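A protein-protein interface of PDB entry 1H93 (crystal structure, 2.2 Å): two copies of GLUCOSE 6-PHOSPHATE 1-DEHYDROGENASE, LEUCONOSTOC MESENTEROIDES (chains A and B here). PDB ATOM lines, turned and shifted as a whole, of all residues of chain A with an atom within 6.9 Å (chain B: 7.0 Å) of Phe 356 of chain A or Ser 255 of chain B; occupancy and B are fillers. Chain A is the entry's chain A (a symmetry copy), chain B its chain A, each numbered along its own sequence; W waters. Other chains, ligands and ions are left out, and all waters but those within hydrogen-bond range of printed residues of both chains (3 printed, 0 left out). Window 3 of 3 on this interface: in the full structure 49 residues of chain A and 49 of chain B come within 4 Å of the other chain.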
ATOM      1  N   ALA A 353     -16.052  -4.281   3.167  1.00  0.00           N
ATOM      2  CA  ALA A 353     -17.245  -3.478   2.922  1.00  0.00           C
ATOM      3  C   ALA A 353     -16.935  -2.014   3.236  1.00  0.00           C
ATOM      4  O   ALA A 353     -16.146  -1.729   4.136  1.00  0.00           O
ATOM      5  CB  ALA A 353     -18.399  -3.974   3.797  1.00  0.00           C
ATOM      6  N   GLY A 354     -17.522  -1.094   2.474  1.00  0.00           N
ATOM      7  CA  GLY A 354     -17.297   0.325   2.707  1.00  0.00           C
ATOM      8  C   GLY A 354     -17.941   0.765   4.004  1.00  0.00           C
ATOM      9  O   GLY A 354     -18.844   0.090   4.501  1.00  0.00           O
ATOM     10  N   THR A 355     -17.444   1.848   4.595  1.00  0.00           N
ATOM     11  CA  THR A 355     -18.007   2.351   5.850  1.00  0.00           C
ATOM     12  C   THR A 355     -18.849   3.629   5.710  1.00  0.00           C
ATOM     13  O   THR A 355     -19.135   4.306   6.703  1.00  0.00           O
ATOM     14  CB  THR A 355     -16.904   2.568   6.909  1.00  0.00           C
ATOM     15  OG1 THR A 355     -15.787   3.242   6.314  1.00  0.00           O
ATOM     16  CG2 THR A 355     -16.448   1.241   7.470  1.00  0.00           C
ATOM     17  N   PHE A 356     -19.233   3.971   4.484  1.00  0.00           N
ATOM     18  CA  PHE A 356     -20.050   5.162   4.259  1.00  0.00           C
ATOM     19  C   PHE A 356     -21.504   4.767   4.437  1.00  0.00           C
ATOM     20  O   PHE A 356     -22.026   3.995   3.645  1.00  0.00           O
ATOM     21  CB  PHE A 356     -19.835   5.721   2.845  1.00  0.00           C
ATOM     22  CG  PHE A 356     -20.670   6.937   2.538  1.00  0.00           C
ATOM     23  CD1 PHE A 356     -20.201   8.214   2.835  1.00  0.00           C
ATOM     24  CD2 PHE A 356     -21.930   6.804   1.957  1.00  0.00           C
ATOM     25  CE1 PHE A 356     -20.977   9.341   2.558  1.00  0.00           C
ATOM     26  CE2 PHE A 356     -22.713   7.925   1.678  1.00  0.00           C
ATOM     27  CZ  PHE A 356     -22.234   9.193   1.978  1.00  0.00           C
ATOM     28  N   ASN A 357     -22.157   5.309   5.459  1.00  0.00           N
ATOM     29  CA  ASN A 357     -23.558   4.988   5.724  1.00  0.00           C
ATOM     30  C   ASN A 357     -24.534   5.811   4.894  1.00  0.00           C
ATOM     31  O   ASN A 357     -24.508   7.043   4.911  1.00  0.00           O
ATOM     32  CB  ASN A 357     -23.890   5.137   7.215  1.00  0.00           C
ATOM     33  CG  ASN A 357     -23.355   3.981   8.063  1.00  0.00           C
ATOM     34  OD1 ASN A 357     -22.936   2.944   7.546  1.00  0.00           O
ATOM     35  ND2 ASN A 357     -23.397   4.151   9.377  1.00  0.00           N
ATOM     36  N   PHE A 358     -25.376   5.109   4.147  1.00  0.00           N
ATOM     37  CA  PHE A 358     -26.390   5.728   3.309  1.00  0.00           C
ATOM     38  C   PHE A 358     -27.676   5.930   4.107  1.00  0.00           C
ATOM     39  O   PHE A 358     -28.607   6.573   3.636  1.00  0.00           O
ATOM     40  CB  PHE A 358     -26.703   4.837   2.106  1.00  0.00           C
ATOM     41  CG  PHE A 358     -25.543   4.637   1.175  1.00  0.00           C
ATOM     42  CD1 PHE A 358     -25.296   5.543   0.147  1.00  0.00           C
ATOM     43  CD2 PHE A 358     -24.714   3.528   1.307  1.00  0.00           C
ATOM     44  CE1 PHE A 358     -24.242   5.347  -0.741  1.00  0.00           C
ATOM     45  CE2 PHE A 358     -23.657   3.321   0.426  1.00  0.00           C
ATOM     46  CZ  PHE A 358     -23.419   4.231  -0.600  1.00  0.00           C
ATOM     47  N   GLY A 359     -27.725   5.357   5.306  1.00  0.00           N
ATOM     48  CA  GLY A 359     -28.908   5.464   6.141  1.00  0.00           C
ATOM     49  C   GLY A 359     -29.997   4.493   5.711  1.00  0.00           C
ATOM     50  O   GLY A 359     -31.153   4.646   6.098  1.00  0.00           O
ATOM     51  N   GLU A 363     -27.027  -1.803   4.336  1.00  0.00           N
ATOM     52  CA  GLU A 363     -25.848  -0.982   4.093  1.00  0.00           C
ATOM     53  C   GLU A 363     -24.903  -1.725   3.145  1.00  0.00           C
ATOM     54  O   GLU A 363     -25.141  -2.887   2.816  1.00  0.00           O
ATOM     55  CB  GLU A 363     -25.143  -0.630   5.403  1.00  0.00           C
ATOM     56  CG  GLU A 363     -25.922   0.336   6.302  1.00  0.00           C
ATOM     57  CD  GLU A 363     -26.112   1.737   5.703  1.00  0.00           C
ATOM     58  OE1 GLU A 363     -25.470   2.082   4.685  1.00  0.00           O
ATOM     59  OE2 GLU A 363     -26.913   2.507   6.274  1.00  0.00           O
ATOM     60  N   ALA A 364     -23.848  -1.051   2.698  1.00  0.00           N
ATOM     61  CA  ALA A 364     -22.881  -1.633   1.771  1.00  0.00           C
ATOM     62  C   ALA A 364     -22.367  -2.990   2.219  1.00  0.00           C
ATOM     63  O   ALA A 364     -22.199  -3.245   3.409  1.00  0.00           O
ATOM     64  CB  ALA A 364     -21.716  -0.682   1.546  1.00  0.00           C
ATOM     65  N   ALA B 189     -24.248   7.416  -6.837  1.00  0.00           N
ATOM     66  CA  ALA B 189     -23.758   7.538  -5.467  1.00  0.00           C
ATOM     67  C   ALA B 189     -23.478   6.177  -4.827  1.00  0.00           C
ATOM     68  O   ALA B 189     -22.490   6.015  -4.110  1.00  0.00           O
ATOM     69  CB  ALA B 189     -24.753   8.317  -4.622  1.00  0.00           C
ATOM     70  N   PHE B 193     -19.698   5.538  -3.507  1.00  0.00           N
ATOM     71  CA  PHE B 193     -19.517   5.427  -2.059  1.00  0.00           C
ATOM     72  C   PHE B 193     -19.746   4.048  -1.471  1.00  0.00           C
ATOM     73  O   PHE B 193     -19.361   3.783  -0.326  1.00  0.00           O
ATOM     74  CB  PHE B 193     -20.422   6.431  -1.334  1.00  0.00           C
ATOM     75  CG  PHE B 193     -20.258   7.839  -1.804  1.00  0.00           C
ATOM     76  CD1 PHE B 193     -19.010   8.446  -1.793  1.00  0.00           C
ATOM     77  CD2 PHE B 193     -21.355   8.554  -2.277  1.00  0.00           C
ATOM     78  CE1 PHE B 193     -18.850   9.744  -2.249  1.00  0.00           C
ATOM     79  CE2 PHE B 193     -21.209   9.856  -2.736  1.00  0.00           C
ATOM     80  CZ  PHE B 193     -19.956  10.452  -2.724  1.00  0.00           C
ATOM     81  N   GLY B 194     -20.438   3.195  -2.212  1.00  0.00           N
ATOM     82  CA  GLY B 194     -20.702   1.856  -1.724  1.00  0.00           C
ATOM     83  C   GLY B 194     -19.563   0.879  -1.970  1.00  0.00           C
ATOM     84  O   GLY B 194     -19.501  -0.169  -1.327  1.00  0.00           O
ATOM     85  N   ASP B 199     -14.686   4.378  -4.749  1.00  0.00           N
ATOM     86  CA  ASP B 199     -14.678   5.533  -3.863  1.00  0.00           C
ATOM     87  C   ASP B 199     -13.276   6.146  -3.785  1.00  0.00           C
ATOM     88  O   ASP B 199     -13.086   7.331  -4.061  1.00  0.00           O
ATOM     89  CB  ASP B 199     -15.154   5.099  -2.470  1.00  0.00           C
ATOM     90  CG  ASP B 199     -15.428   6.278  -1.528  1.00  0.00           C
ATOM     91  OD1 ASP B 199     -15.463   7.444  -1.974  1.00  0.00           O
ATOM     92  OD2 ASP B 199     -15.628   6.028  -0.325  1.00  0.00           O
ATOM     93  N   MET B 250     -19.276  15.815  -7.352  1.00  0.00           N
ATOM     94  CA  MET B 250     -19.405  16.163  -5.944  1.00  0.00           C
ATOM     95  C   MET B 250     -18.268  15.602  -5.108  1.00  0.00           C
ATOM     96  O   MET B 250     -17.590  14.649  -5.505  1.00  0.00           O
ATOM     97  CB  MET B 250     -20.743  15.671  -5.380  1.00  0.00           C
ATOM     98  CG  MET B 250     -20.896  14.165  -5.366  1.00  0.00           C
ATOM     99  SD  MET B 250     -22.472  13.596  -4.749  1.00  0.00           S
ATOM    100  CE  MET B 250     -22.329  14.015  -3.057  1.00  0.00           C
ATOM    101  N   LYS B 252     -16.911  13.974  -1.405  1.00  0.00           N
ATOM    102  CA  LYS B 252     -17.506  12.918  -0.607  1.00  0.00           C
ATOM    103  C   LYS B 252     -18.179  13.637   0.557  1.00  0.00           C
ATOM    104  O   LYS B 252     -17.513  14.339   1.320  1.00  0.00           O
ATOM    105  CB  LYS B 252     -16.448  11.947  -0.090  1.00  0.00           C
ATOM    106  CG  LYS B 252     -17.032  10.829   0.756  1.00  0.00           C
ATOM    107  CD  LYS B 252     -16.023   9.717   0.969  1.00  0.00           C
ATOM    108  CE  LYS B 252     -16.605   8.617   1.834  1.00  0.00           C
ATOM    109  NZ  LYS B 252     -15.606   7.561   2.116  1.00  0.00           N
ATOM    110  N   PRO B 253     -19.518  13.525   0.668  1.00  0.00           N
ATOM    111  CA  PRO B 253     -20.278  14.174   1.742  1.00  0.00           C
ATOM    112  C   PRO B 253     -19.979  13.584   3.109  1.00  0.00           C
ATOM    113  O   PRO B 253     -19.416  12.495   3.215  1.00  0.00           O
ATOM    114  CB  PRO B 253     -21.725  13.921   1.326  1.00  0.00           C
ATOM    115  CG  PRO B 253     -21.646  12.593   0.653  1.00  0.00           C
ATOM    116  CD  PRO B 253     -20.419  12.749  -0.203  1.00  0.00           C
ATOM    117  N   GLU B 254     -20.380  14.294   4.157  1.00  0.00           N
ATOM    118  CA  GLU B 254     -20.142  13.825   5.515  1.00  0.00           C
ATOM    119  C   GLU B 254     -21.207  12.866   6.022  1.00  0.00           C
ATOM    120  O   GLU B 254     -21.122  12.369   7.141  1.00  0.00           O
ATOM    121  CB  GLU B 254     -19.942  15.010   6.456  1.00  0.00           C
ATOM    122  CG  GLU B 254     -18.543  15.604   6.315  1.00  0.00           C
ATOM    123  CD  GLU B 254     -18.447  17.058   6.728  1.00  0.00           C
ATOM    124  OE1 GLU B 254     -19.129  17.460   7.699  1.00  0.00           O
ATOM    125  OE2 GLU B 254     -17.674  17.798   6.077  1.00  0.00           O
ATOM    126  N   SER B 255     -22.218  12.628   5.199  1.00  0.00           N
ATOM    127  CA  SER B 255     -23.301  11.701   5.512  1.00  0.00           C
ATOM    128  C   SER B 255     -24.157  11.665   4.260  1.00  0.00           C
ATOM    129  O   SER B 255     -23.833  12.333   3.277  1.00  0.00           O
ATOM    130  CB  SER B 255     -24.119  12.159   6.735  1.00  0.00           C
ATOM    131  OG  SER B 255     -25.084  13.157   6.415  1.00  0.00           O
ATOM    132  N   PHE B 256     -25.230  10.886   4.264  1.00  0.00           N
ATOM    133  CA  PHE B 256     -26.067  10.837   3.079  1.00  0.00           C
ATOM    134  C   PHE B 256     -27.364  11.652   3.190  1.00  0.00           C
ATOM    135  O   PHE B 256     -28.350  11.355   2.510  1.00  0.00           O
ATOM    136  CB  PHE B 256     -26.355   9.393   2.663  1.00  0.00           C
ATOM    137  CG  PHE B 256     -26.580   9.232   1.187  1.00  0.00           C
ATOM    138  CD1 PHE B 256     -25.655   9.734   0.274  1.00  0.00           C
ATOM    139  CD2 PHE B 256     -27.722   8.604   0.707  1.00  0.00           C
ATOM    140  CE1 PHE B 256     -25.867   9.615  -1.105  1.00  0.00           C
ATOM    141  CE2 PHE B 256     -27.946   8.479  -0.665  1.00  0.00           C
ATOM    142  CZ  PHE B 256     -27.014   8.987  -1.575  1.00  0.00           C
ATOM    143  N   THR B 257     -27.371  12.666   4.053  1.00  0.00           N
ATOM    144  CA  THR B 257     -28.554  13.511   4.179  1.00  0.00           C
ATOM    145  C   THR B 257     -28.506  14.461   2.987  1.00  0.00           C
ATOM    146  O   THR B 257     -27.418  14.825   2.524  1.00  0.00           O
ATOM    147  CB  THR B 257     -28.551  14.344   5.484  1.00  0.00           C
ATOM    148  OG1 THR B 257     -27.417  15.221   5.505  1.00  0.00           O
ATOM    149  CG2 THR B 257     -28.519  13.438   6.705  1.00  0.00           C
ATOM    150  N   ASP B 258     -29.669  14.857   2.478  1.00  0.00           N
ATOM    151  CA  ASP B 258     -29.723  15.778   1.337  1.00  0.00           C
ATOM    152  C   ASP B 258     -28.933  17.076   1.575  1.00  0.00           C
ATOM    153  O   ASP B 258     -28.390  17.665   0.642  1.00  0.00           O
ATOM    154  CB  ASP B 258     -31.181  16.071   0.919  1.00  0.00           C
ATOM    155  CG  ASP B 258     -32.097  16.406   2.097  1.00  0.00           C
ATOM    156  OD1 ASP B 258     -31.610  16.575   3.235  1.00  0.00           O
ATOM    157  OD2 ASP B 258     -33.326  16.508   1.881  1.00  0.00           O
ATOM    158  N   LYS B 259     -28.822  17.472   2.841  1.00  0.00           N
ATOM    159  CA  LYS B 259     -28.093  18.676   3.235  1.00  0.00           C
ATOM    160  C   LYS B 259     -26.602  18.517   2.920  1.00  0.00           C
ATOM    161  O   LYS B 259     -26.002  19.375   2.259  1.00  0.00           O
ATOM    162  CB  LYS B 259     -28.300  18.937   4.731  1.00  0.00           C
ATOM    163  CG  LYS B 259     -27.615  20.184   5.284  1.00  0.00           C
ATOM    164  CD  LYS B 259     -27.778  20.245   6.806  1.00  0.00           C
ATOM    165  CE  LYS B 259     -26.946  21.351   7.456  1.00  0.00           C
ATOM    166  NZ  LYS B 259     -27.392  22.721   7.083  1.00  0.00           N
ATOM    167  N   ASP B 260     -26.020  17.398   3.359  1.00  0.00           N
ATOM    168  CA  ASP B 260     -24.602  17.114   3.123  1.00  0.00           C
ATOM    169  C   ASP B 260     -24.328  16.791   1.660  1.00  0.00           C
ATOM    170  O   ASP B 260     -23.256  17.111   1.130  1.00  0.00           O
ATOM    171  CB  ASP B 260     -24.120  15.994   4.042  1.00  0.00           C
ATOM    172  CG  ASP B 260     -24.068  16.426   5.510  1.00  0.00           C
ATOM    173  OD1 ASP B 260     -24.098  17.646   5.779  1.00  0.00           O
ATOM    174  OD2 ASP B 260     -23.980  15.546   6.385  1.00  0.00           O
ATOM    175  N   ILE B 261     -25.311  16.188   1.000  1.00  0.00           N
ATOM    176  CA  ILE B 261     -25.193  15.870  -0.417  1.00  0.00           C
ATOM    177  C   ILE B 261     -25.092  17.188  -1.181  1.00  0.00           C
ATOM    178  O   ILE B 261     -24.159  17.394  -1.961  1.00  0.00           O
ATOM    179  CB  ILE B 261     -26.441  15.095  -0.913  1.00  0.00           C
ATOM    180  CG1 ILE B 261     -26.497  13.722  -0.242  1.00  0.00           C
ATOM    181  CG2 ILE B 261     -26.436  14.948  -2.424  1.00  0.00           C
ATOM    182  CD1 ILE B 261     -27.726  12.925  -0.617  1.00  0.00           C
HETATM  183  O   HOH W   1     -16.503   6.070   4.476  1.00  0.00           O
HETATM  184  O   HOH W   2     -18.352  -2.136  -0.067  1.00  0.00           O
HETATM  185  O   HOH W   3     -19.827   2.429   1.893  1.00  0.00           O
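Of chain B, only Phe 193, Lys 252, Pro 253, Ser 255 and Phe 256 come within 4 Å of Phe 356 of chain A. Of chain A, only Phe 356 (3.8 Å) comes within 4 Å of Ser 255 of chain B. Of the printed residues of chain B, Phe 358 of chain A touches Ala 189 (3.9 Å), Phe 193 (3.8 Å), Gly 194 (3.5 Å) and Phe 256 (3.7 Å). Of the printed residues of chain A, Lys 252 of chain B touches Phe 356 (3.8 Å). Printed residues of chain A within 4 Å of Gly 194 of chain B: Phe 358 and Ala 364. Gly 359 of chain A touches none of the printed residues of chain B.
Water W2 bridges O of Gly 194 of chain B and N of Gly 354 of chain A. Water W3 lies within hydrogen-bond range of the backbone carbonyl oxygen (O) of Phe 193 of chain B (2.6 Å) and the backbone NH (N) of Phe 356 of chain A (3.1 Å). Water W1 lies within hydrogen-bond range of the side-chain amino group (NZ) of Lys 252 of chain B, the backbone NH (N) of Phe 356 of chain A and the side-chain hydroxyl (OG1) of Thr 355 of chain A.
Of the 15 printed residues of chain B, 7 touch a printed residue of chain A. Of the 9 printed residues of chain A, 4 touch a printed residue of chain B. Printed residues of chain A that touch a printed residue of chain B: Phe 356, Asn 357, Phe 358 and Ala 364. Hydrophobic or aromatic side chains of chain A that line the printed part of chain B: Phe 356, Phe 358 and Ala 364.
The side-chain carboxylate of Asp 199 of chain B lies within salt-bridge range of the side-chain amino group of Lys 252 of chain B, 2.9 Å away. OG1 of Thr 257 of chain B is in hydrogen-bond range of OG of Ser 255 of chain B, at 3.2 Å. OD2 of Asp 260 of chain B sits at hydrogen-bond distance from OG of Ser 255 of chain B, 2.6 Å away. The side-chain carboxylate of Glu 363 of chain A lies within hydrogen-bond range of the backbone NH of Phe 358 of chain A (3.1 Å).
No position is printed for both chains.
Among the printed residues, merely in contact across the chains: Phe 358 of chain A with Gly 194 of chain B, Phe 356 of chain A with Pro 253 of chain B, Phe 356 of chain A with Phe 193 of chain B, Ala 364 of chain A with Gly 194 of chain B, Phe 358 of chain A with Phe 256 of chain B, Phe 356 of chain A with Phe 256 of chain B, Asn 357 of chain A with Phe 256 of chain B, Phe 356 of chain A with Lys 252 of chain B, Phe 356 of chain A with Ser 255 of chain B, Phe 358 of chain A with Phe 193 of chain B and Phe 358 of chain A with Ala 189 of chain B.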
